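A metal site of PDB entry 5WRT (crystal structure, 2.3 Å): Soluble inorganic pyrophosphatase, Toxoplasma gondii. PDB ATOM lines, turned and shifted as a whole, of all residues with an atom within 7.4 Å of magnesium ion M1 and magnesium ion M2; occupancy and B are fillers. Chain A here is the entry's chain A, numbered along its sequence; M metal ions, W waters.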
ATOM      1  N   GLU A  52      21.419  14.049 -20.679  1.00  0.00           N
ATOM      2  CA  GLU A  52      21.581  13.770 -19.264  1.00  0.00           C
ATOM      3  C   GLU A  52      22.592  12.668 -18.999  1.00  0.00           C
ATOM      4  O   GLU A  52      23.477  12.820 -18.145  1.00  0.00           O
ATOM      5  CB  GLU A  52      20.229  13.393 -18.637  1.00  0.00           C
ATOM      6  CG  GLU A  52      19.196  14.513 -18.630  1.00  0.00           C
ATOM      7  CD  GLU A  52      17.824  14.043 -18.183  1.00  0.00           C
ATOM      8  OE1 GLU A  52      17.482  12.869 -18.433  1.00  0.00           O
ATOM      9  OE2 GLU A  52      17.080  14.856 -17.592  1.00  0.00           O
ATOM     10  N   MET A  61      22.001  10.271 -14.159  1.00  0.00           N
ATOM     11  CA  MET A  61      21.936  11.727 -14.160  1.00  0.00           C
ATOM     12  C   MET A  61      20.595  12.172 -14.723  1.00  0.00           C
ATOM     13  O   MET A  61      20.123  11.664 -15.736  1.00  0.00           O
ATOM     14  CB  MET A  61      23.080  12.309 -14.985  1.00  0.00           C
ATOM     15  CG  MET A  61      24.442  11.754 -14.632  1.00  0.00           C
ATOM     16  SD  MET A  61      24.970  12.142 -12.953  1.00  0.00           S
ATOM     17  CE  MET A  61      25.058  13.917 -13.020  1.00  0.00           C
ATOM     18  N   GLU A  62      19.985  13.168 -14.062  1.00  0.00           N
ATOM     19  CA  GLU A  62      18.684  13.667 -14.483  1.00  0.00           C
ATOM     20  C   GLU A  62      18.555  15.127 -14.102  1.00  0.00           C
ATOM     21  O   GLU A  62      19.162  15.586 -13.133  1.00  0.00           O
ATOM     22  CB  GLU A  62      17.527  12.889 -13.848  1.00  0.00           C
ATOM     23  CG  GLU A  62      17.366  11.445 -14.296  1.00  0.00           C
ATOM     24  CD  GLU A  62      16.306  10.707 -13.510  1.00  0.00           C
ATOM     25  OE1 GLU A  62      15.912  11.191 -12.428  1.00  0.00           O
ATOM     26  OE2 GLU A  62      15.861   9.640 -13.989  1.00  0.00           O
ATOM     27  N   MET A  63      17.758  15.857 -14.871  1.00  0.00           N
ATOM     28  CA  MET A  63      17.371  17.205 -14.493  1.00  0.00           C
ATOM     29  C   MET A  63      16.574  17.167 -13.186  1.00  0.00           C
ATOM     30  O   MET A  63      15.630  16.380 -13.042  1.00  0.00           O
ATOM     31  CB  MET A  63      16.528  17.853 -15.597  1.00  0.00           C
ATOM     32  CG  MET A  63      17.312  18.144 -16.866  1.00  0.00           C
ATOM     33  SD  MET A  63      16.350  19.068 -18.089  1.00  0.00           S
ATOM     34  CE  MET A  63      15.219  17.800 -18.670  1.00  0.00           C
ATOM     35  N   TYR A  85      22.277   2.972 -12.903  1.00  0.00           N
ATOM     36  CA  TYR A  85      21.643   1.850 -13.577  1.00  0.00           C
ATOM     37  C   TYR A  85      22.500   0.603 -13.397  1.00  0.00           C
ATOM     38  O   TYR A  85      23.717   0.673 -13.239  1.00  0.00           O
ATOM     39  CB  TYR A  85      21.440   2.151 -15.067  1.00  0.00           C
ATOM     40  CG  TYR A  85      20.351   3.160 -15.337  1.00  0.00           C
ATOM     41  CD1 TYR A  85      19.109   3.042 -14.724  1.00  0.00           C
ATOM     42  CD2 TYR A  85      20.561   4.221 -16.200  1.00  0.00           C
ATOM     43  CE1 TYR A  85      18.100   3.964 -14.968  1.00  0.00           C
ATOM     44  CE2 TYR A  85      19.561   5.151 -16.449  1.00  0.00           C
ATOM     45  CZ  TYR A  85      18.329   5.016 -15.828  1.00  0.00           C
ATOM     46  OH  TYR A  85      17.340   5.927 -16.069  1.00  0.00           O
ATOM     47  N   TYR A  93      21.688   9.765 -23.910  1.00  0.00           N
ATOM     48  CA  TYR A  93      20.331   9.673 -23.422  1.00  0.00           C
ATOM     49  C   TYR A  93      19.972  10.943 -22.665  1.00  0.00           C
ATOM     50  O   TYR A  93      20.804  11.496 -21.935  1.00  0.00           O
ATOM     51  CB  TYR A  93      20.173   8.439 -22.521  1.00  0.00           C
ATOM     52  CG  TYR A  93      18.789   8.214 -21.956  1.00  0.00           C
ATOM     53  CD1 TYR A  93      17.780   7.698 -22.746  1.00  0.00           C
ATOM     54  CD2 TYR A  93      18.503   8.491 -20.630  1.00  0.00           C
ATOM     55  CE1 TYR A  93      16.508   7.474 -22.242  1.00  0.00           C
ATOM     56  CE2 TYR A  93      17.239   8.280 -20.106  1.00  0.00           C
ATOM     57  CZ  TYR A  93      16.249   7.765 -20.919  1.00  0.00           C
ATOM     58  OH  TYR A  93      14.988   7.546 -20.406  1.00  0.00           O
ATOM     59  N   GLY A  94      18.732  11.397 -22.823  1.00  0.00           N
ATOM     60  CA  GLY A  94      18.290  12.607 -22.180  1.00  0.00           C
ATOM     61  C   GLY A  94      16.810  12.872 -22.341  1.00  0.00           C
ATOM     62  O   GLY A  94      16.006  11.939 -22.294  1.00  0.00           O
ATOM     63  N   ALA A  95      16.440  14.136 -22.535  1.00  0.00           N
ATOM     64  CA  ALA A  95      15.037  14.500 -22.559  1.00  0.00           C
ATOM     65  C   ALA A  95      14.834  15.716 -23.456  1.00  0.00           C
ATOM     66  O   ALA A  95      15.766  16.479 -23.731  1.00  0.00           O
ATOM     67  CB  ALA A  95      14.506  14.777 -21.155  1.00  0.00           C
ATOM     68  N   GLU A 101       5.162  14.355 -19.837  1.00  0.00           N
ATOM     69  CA  GLU A 101       4.281  13.220 -20.103  1.00  0.00           C
ATOM     70  C   GLU A 101       3.197  13.211 -19.017  1.00  0.00           C
ATOM     71  O   GLU A 101       3.250  12.467 -18.032  1.00  0.00           O
ATOM     72  CB  GLU A 101       5.054  11.919 -20.171  1.00  0.00           C
ATOM     73  CG  GLU A 101       5.866  11.789 -21.445  1.00  0.00           C
ATOM     74  CD  GLU A 101       5.037  11.276 -22.608  1.00  0.00           C
ATOM     75  OE1 GLU A 101       4.860  10.044 -22.730  1.00  0.00           O
ATOM     76  OE2 GLU A 101       4.542  12.118 -23.390  1.00  0.00           O
ATOM     77  N   GLY A 116       0.756   8.547 -18.601  1.00  0.00           N
ATOM     78  CA  GLY A 116       2.039   9.223 -18.746  1.00  0.00           C
ATOM     79  C   GLY A 116       2.954   8.972 -17.563  1.00  0.00           C
ATOM     80  O   GLY A 116       2.517   8.800 -16.426  1.00  0.00           O
ATOM     81  N   ASP A 117       4.273   8.956 -17.850  1.00  0.00           N
ATOM     82  CA  ASP A 117       5.287   8.720 -16.807  1.00  0.00           C
ATOM     83  C   ASP A 117       5.460   9.903 -15.869  1.00  0.00           C
ATOM     84  O   ASP A 117       6.141   9.762 -14.846  1.00  0.00           O
ATOM     85  CB  ASP A 117       6.646   8.381 -17.455  1.00  0.00           C
ATOM     86  CG  ASP A 117       7.430   9.611 -17.985  1.00  0.00           C
ATOM     87  OD1 ASP A 117       8.627   9.483 -18.329  1.00  0.00           O
ATOM     88  OD2 ASP A 117       6.894  10.751 -17.983  1.00  0.00           O
ATOM     89  N   GLY A 118       4.905  11.064 -16.199  1.00  0.00           N
ATOM     90  CA  GLY A 118       5.026  12.220 -15.347  1.00  0.00           C
ATOM     91  C   GLY A 118       6.318  13.002 -15.481  1.00  0.00           C
ATOM     92  O   GLY A 118       6.481  14.012 -14.770  1.00  0.00           O
ATOM     93  N   ASP A 119       7.232  12.581 -16.346  1.00  0.00           N
ATOM     94  CA  ASP A 119       8.527  13.206 -16.549  1.00  0.00           C
ATOM     95  C   ASP A 119       8.624  13.869 -17.924  1.00  0.00           C
ATOM     96  O   ASP A 119       7.755  13.677 -18.778  1.00  0.00           O
ATOM     97  CB  ASP A 119       9.640  12.167 -16.405  1.00  0.00           C
ATOM     98  CG  ASP A 119      10.248  12.143 -15.016  1.00  0.00           C
ATOM     99  OD1 ASP A 119       9.748  12.890 -14.150  1.00  0.00           O
ATOM    100  OD2 ASP A 119      11.223  11.399 -14.809  1.00  0.00           O
ATOM    101  N   PRO A 120       9.654  14.682 -18.164  1.00  0.00           N
ATOM    102  CA  PRO A 120       9.931  15.123 -19.536  1.00  0.00           C
ATOM    103  C   PRO A 120      10.189  13.935 -20.458  1.00  0.00           C
ATOM    104  O   PRO A 120      10.726  12.908 -20.044  1.00  0.00           O
ATOM    105  CB  PRO A 120      11.188  15.995 -19.391  1.00  0.00           C
ATOM    106  CG  PRO A 120      11.152  16.463 -17.986  1.00  0.00           C
ATOM    107  CD  PRO A 120      10.498  15.383 -17.179  1.00  0.00           C
ATOM    108  N   LEU A 121       9.797  14.097 -21.718  1.00  0.00           N
ATOM    109  CA  LEU A 121       9.859  12.989 -22.675  1.00  0.00           C
ATOM    110  C   LEU A 121      11.300  12.566 -22.924  1.00  0.00           C
ATOM    111  O   LEU A 121      12.170  13.400 -23.170  1.00  0.00           O
ATOM    112  CB  LEU A 121       9.193  13.408 -23.992  1.00  0.00           C
ATOM    113  CG  LEU A 121       9.136  12.345 -25.090  1.00  0.00           C
ATOM    114  CD1 LEU A 121       8.378  11.121 -24.602  1.00  0.00           C
ATOM    115  CD2 LEU A 121       8.500  12.908 -26.335  1.00  0.00           C
ATOM    116  N   ASP A 122      11.538  11.256 -22.861  1.00  0.00           N
ATOM    117  CA  ASP A 122      12.876  10.704 -22.992  1.00  0.00           C
ATOM    118  C   ASP A 122      13.251  10.526 -24.462  1.00  0.00           C
ATOM    119  O   ASP A 122      12.410  10.239 -25.309  1.00  0.00           O
ATOM    120  CB  ASP A 122      12.974   9.350 -22.284  1.00  0.00           C
ATOM    121  CG  ASP A 122      12.594   9.430 -20.822  1.00  0.00           C
ATOM    122  OD1 ASP A 122      13.040  10.370 -20.133  1.00  0.00           O
ATOM    123  OD2 ASP A 122      11.847   8.552 -20.352  1.00  0.00           O
ATOM    124  N   VAL A 123      14.539  10.707 -24.755  1.00  0.00           N
ATOM    125  CA  VAL A 123      15.062  10.562 -26.107  1.00  0.00           C
ATOM    126  C   VAL A 123      16.408   9.843 -26.053  1.00  0.00           C
ATOM    127  O   VAL A 123      17.248  10.125 -25.194  1.00  0.00           O
ATOM    128  CB  VAL A 123      15.191  11.922 -26.831  1.00  0.00           C
ATOM    129  CG1 VAL A 123      16.007  12.908 -25.992  1.00  0.00           C
ATOM    130  CG2 VAL A 123      15.801  11.755 -28.216  1.00  0.00           C
ATOM    131  N   MET A 147       7.647   1.789 -24.326  1.00  0.00           N
ATOM    132  CA  MET A 147       7.915   0.939 -23.173  1.00  0.00           C
ATOM    133  C   MET A 147       6.868   1.173 -22.099  1.00  0.00           C
ATOM    134  O   MET A 147       6.449   2.307 -21.849  1.00  0.00           O
ATOM    135  CB  MET A 147       9.333   1.199 -22.647  1.00  0.00           C
ATOM    136  CG  MET A 147       9.858   0.115 -21.716  1.00  0.00           C
ATOM    137  SD  MET A 147      11.127   0.681 -20.553  1.00  0.00           S
ATOM    138  CE  MET A 147      10.176   1.718 -19.470  1.00  0.00           C
ATOM    139  N   GLU A 152       2.882   2.496 -16.446  1.00  0.00           N
ATOM    140  CA  GLU A 152       3.227   3.819 -16.943  1.00  0.00           C
ATOM    141  C   GLU A 152       3.767   3.704 -18.360  1.00  0.00           C
ATOM    142  O   GLU A 152       4.632   2.869 -18.634  1.00  0.00           O
ATOM    143  CB  GLU A 152       4.270   4.505 -16.064  1.00  0.00           C
ATOM    144  CG  GLU A 152       3.776   4.926 -14.688  1.00  0.00           C
ATOM    145  CD  GLU A 152       4.703   5.938 -14.030  1.00  0.00           C
ATOM    146  OE1 GLU A 152       5.932   5.842 -14.225  1.00  0.00           O
ATOM    147  OE2 GLU A 152       4.195   6.846 -13.336  1.00  0.00           O
ATOM    148  N   LEU A 153       3.243   4.535 -19.260  1.00  0.00           N
ATOM    149  CA  LEU A 153       3.773   4.627 -20.611  1.00  0.00           C
ATOM    150  C   LEU A 153       5.047   5.452 -20.599  1.00  0.00           C
ATOM    151  O   LEU A 153       5.024   6.639 -20.242  1.00  0.00           O
ATOM    152  CB  LEU A 153       2.732   5.243 -21.544  1.00  0.00           C
ATOM    153  CG  LEU A 153       3.147   5.543 -22.987  1.00  0.00           C
ATOM    154  CD1 LEU A 153       3.751   4.310 -23.649  1.00  0.00           C
ATOM    155  CD2 LEU A 153       1.947   6.033 -23.785  1.00  0.00           C
ATOM    156  N   ASP A 154       6.164   4.837 -20.965  1.00  0.00           N
ATOM    157  CA  ASP A 154       7.480   5.475 -20.897  1.00  0.00           C
ATOM    158  C   ASP A 154       8.107   5.407 -22.290  1.00  0.00           C
ATOM    159  O   ASP A 154       8.901   4.507 -22.589  1.00  0.00           O
ATOM    160  CB  ASP A 154       8.355   4.783 -19.833  1.00  0.00           C
ATOM    161  CG  ASP A 154       9.690   5.468 -19.641  1.00  0.00           C
ATOM    162  OD1 ASP A 154       9.854   6.622 -20.104  1.00  0.00           O
ATOM    163  OD2 ASP A 154      10.576   4.861 -19.015  1.00  0.00           O
ATOM    164  N   TRP A 155       7.749   6.367 -23.133  1.00  0.00           N
ATOM    165  CA  TRP A 155       8.289   6.424 -24.491  1.00  0.00           C
ATOM    166  C   TRP A 155       9.794   6.582 -24.476  1.00  0.00           C
ATOM    167  O   TRP A 155      10.353   7.308 -23.644  1.00  0.00           O
ATOM    168  CB  TRP A 155       7.664   7.590 -25.266  1.00  0.00           C
ATOM    169  CG  TRP A 155       6.239   7.432 -25.662  1.00  0.00           C
ATOM    170  CD1 TRP A 155       5.158   7.984 -25.055  1.00  0.00           C
ATOM    171  CD2 TRP A 155       5.735   6.679 -26.777  1.00  0.00           C
ATOM    172  NE1 TRP A 155       4.010   7.625 -25.721  1.00  0.00           N
ATOM    173  CE2 TRP A 155       4.337   6.822 -26.767  1.00  0.00           C
ATOM    174  CE3 TRP A 155       6.333   5.897 -27.772  1.00  0.00           C
ATOM    175  CZ2 TRP A 155       3.521   6.214 -27.724  1.00  0.00           C
ATOM    176  CZ3 TRP A 155       5.521   5.292 -28.713  1.00  0.00           C
ATOM    177  CH2 TRP A 155       4.130   5.448 -28.682  1.00  0.00           C
ATOM    178  N   LYS A 156      10.458   5.894 -25.397  1.00  0.00           N
ATOM    179  CA  LYS A 156      11.877   6.128 -25.693  1.00  0.00           C
ATOM    180  C   LYS A 156      11.959   6.544 -27.155  1.00  0.00           C
ATOM    181  O   LYS A 156      11.931   5.703 -28.060  1.00  0.00           O
ATOM    182  CB  LYS A 156      12.706   4.884 -25.405  1.00  0.00           C
ATOM    183  CG  LYS A 156      12.548   4.337 -24.000  1.00  0.00           C
ATOM    184  CD  LYS A 156      12.921   5.377 -22.961  1.00  0.00           C
ATOM    185  CE  LYS A 156      12.753   4.843 -21.551  1.00  0.00           C
ATOM    186  NZ  LYS A 156      12.662   5.926 -20.527  1.00  0.00           N
HETATM  187 MG    MG M   1       9.958   8.570 -19.686  1.00  0.00          MG
HETATM  188 MG    MG M   2      14.059  10.935 -18.353  1.00  0.00          MG
HETATM  189  O   HOH W   1      13.109  12.690 -18.447  1.00  0.00           O
HETATM  190  O   HOH W   2      15.699  11.224 -19.647  1.00  0.00           O
HETATM  191  O   HOH W   3       9.218   8.967 -21.877  1.00  0.00           O
HETATM  192  O   HOH W   4      10.728   8.085 -17.804  1.00  0.00           O
HETATM  193  O   HOH W   5      15.165  11.500 -16.695  1.00  0.00           O
HETATM  194  O   HOH W   6      14.575   8.773 -18.147  1.00  0.00           O
HETATM  195  O   HOH W   7      10.023  10.786 -19.597  1.00  0.00           O
HETATM  196  O   HOH W   8      12.532  10.132 -17.299  1.00  0.00           O
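Magnesium ion M1 is bound by OD1 of Asp 154 (2.0 Å), OD2 of Asp 122 (2.0 Å), water W4 (2.1 Å), OD1 of Asp 117 (2.1 Å), water W7 (2.2 Å) and water W3 (2.3 Å).
Residues that only touch magnesium ion M2: Glu 52.
Two residues have an atom within 4 Å of magnesium ion M2: Glu 52 and Asp 122.
OD2 of Asp 154 is in salt-bridge range of NZ of Lys 156 (2.8 Å).
N of Asp 154 sits at hydrogen-bond distance from O of Met 147 (2.7 Å).
The side-chain carboxylate (OD2) of Asp 122 lies close to the side-chain amino group (NZ) of Lys 156 (2.8 Å).
OD2 of Asp 122 sits close to OH of Tyr 93 (3.3 Å).
The backbone NH (N) of Asp 117 sits at hydrogen-bond distance from the backbone carbonyl oxygen (O) of Leu 153 (3.4 Å).
The side-chain hydroxyl of Tyr 93 lies within hydrogen-bond range of the side-chain amino group of Lys 156 (2.8 Å).
The backbone NH (N) of Glu 52 sits at hydrogen-bond distance from the backbone carbonyl oxygen (O) of Tyr 93, 2.9 Å away.
The side-chain carboxylate (OE2) of Glu 52 sits at hydrogen-bond distance from the backbone NH (N) of Met 63, at 3.0 Å.
Magnesium ion M2 is bound by water W1 (2.0 Å), water W8 (2.0 Å), water W5 (2.1 Å), water W2 (2.1 Å), the side-chain carboxylate (OD1) of Asp 122 (2.1 Å) and water W6 (2.2 Å).
Magnesium ion M2 has six donor atoms within binding distance.
Merely in contact with magnesium ion M1: Lys 156 (3.9 Å).
Within 4 Å of magnesium ion M1: Asp 117, Asp 122, Asp 154 and Lys 156.
The nearest printed residue that does not touch magnesium ion M1 is Trp 155 (4.2 Å).
Water W3 lies within hydrogen-bond range of O of Trp 155 (2.7 Å) and N of Asp 122 (3.4 Å).
Water W5 bridges the side-chain carboxylate of Glu 52 (3.2 Å) and the side-chain carboxylate of Glu 62 (3.4 Å).
Water W2 lies within hydrogen-bond range of the side-chain carboxylate of Glu 52 (2.7 Å) and the backbone carbonyl oxygen of Gly 94 (2.8 Å).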
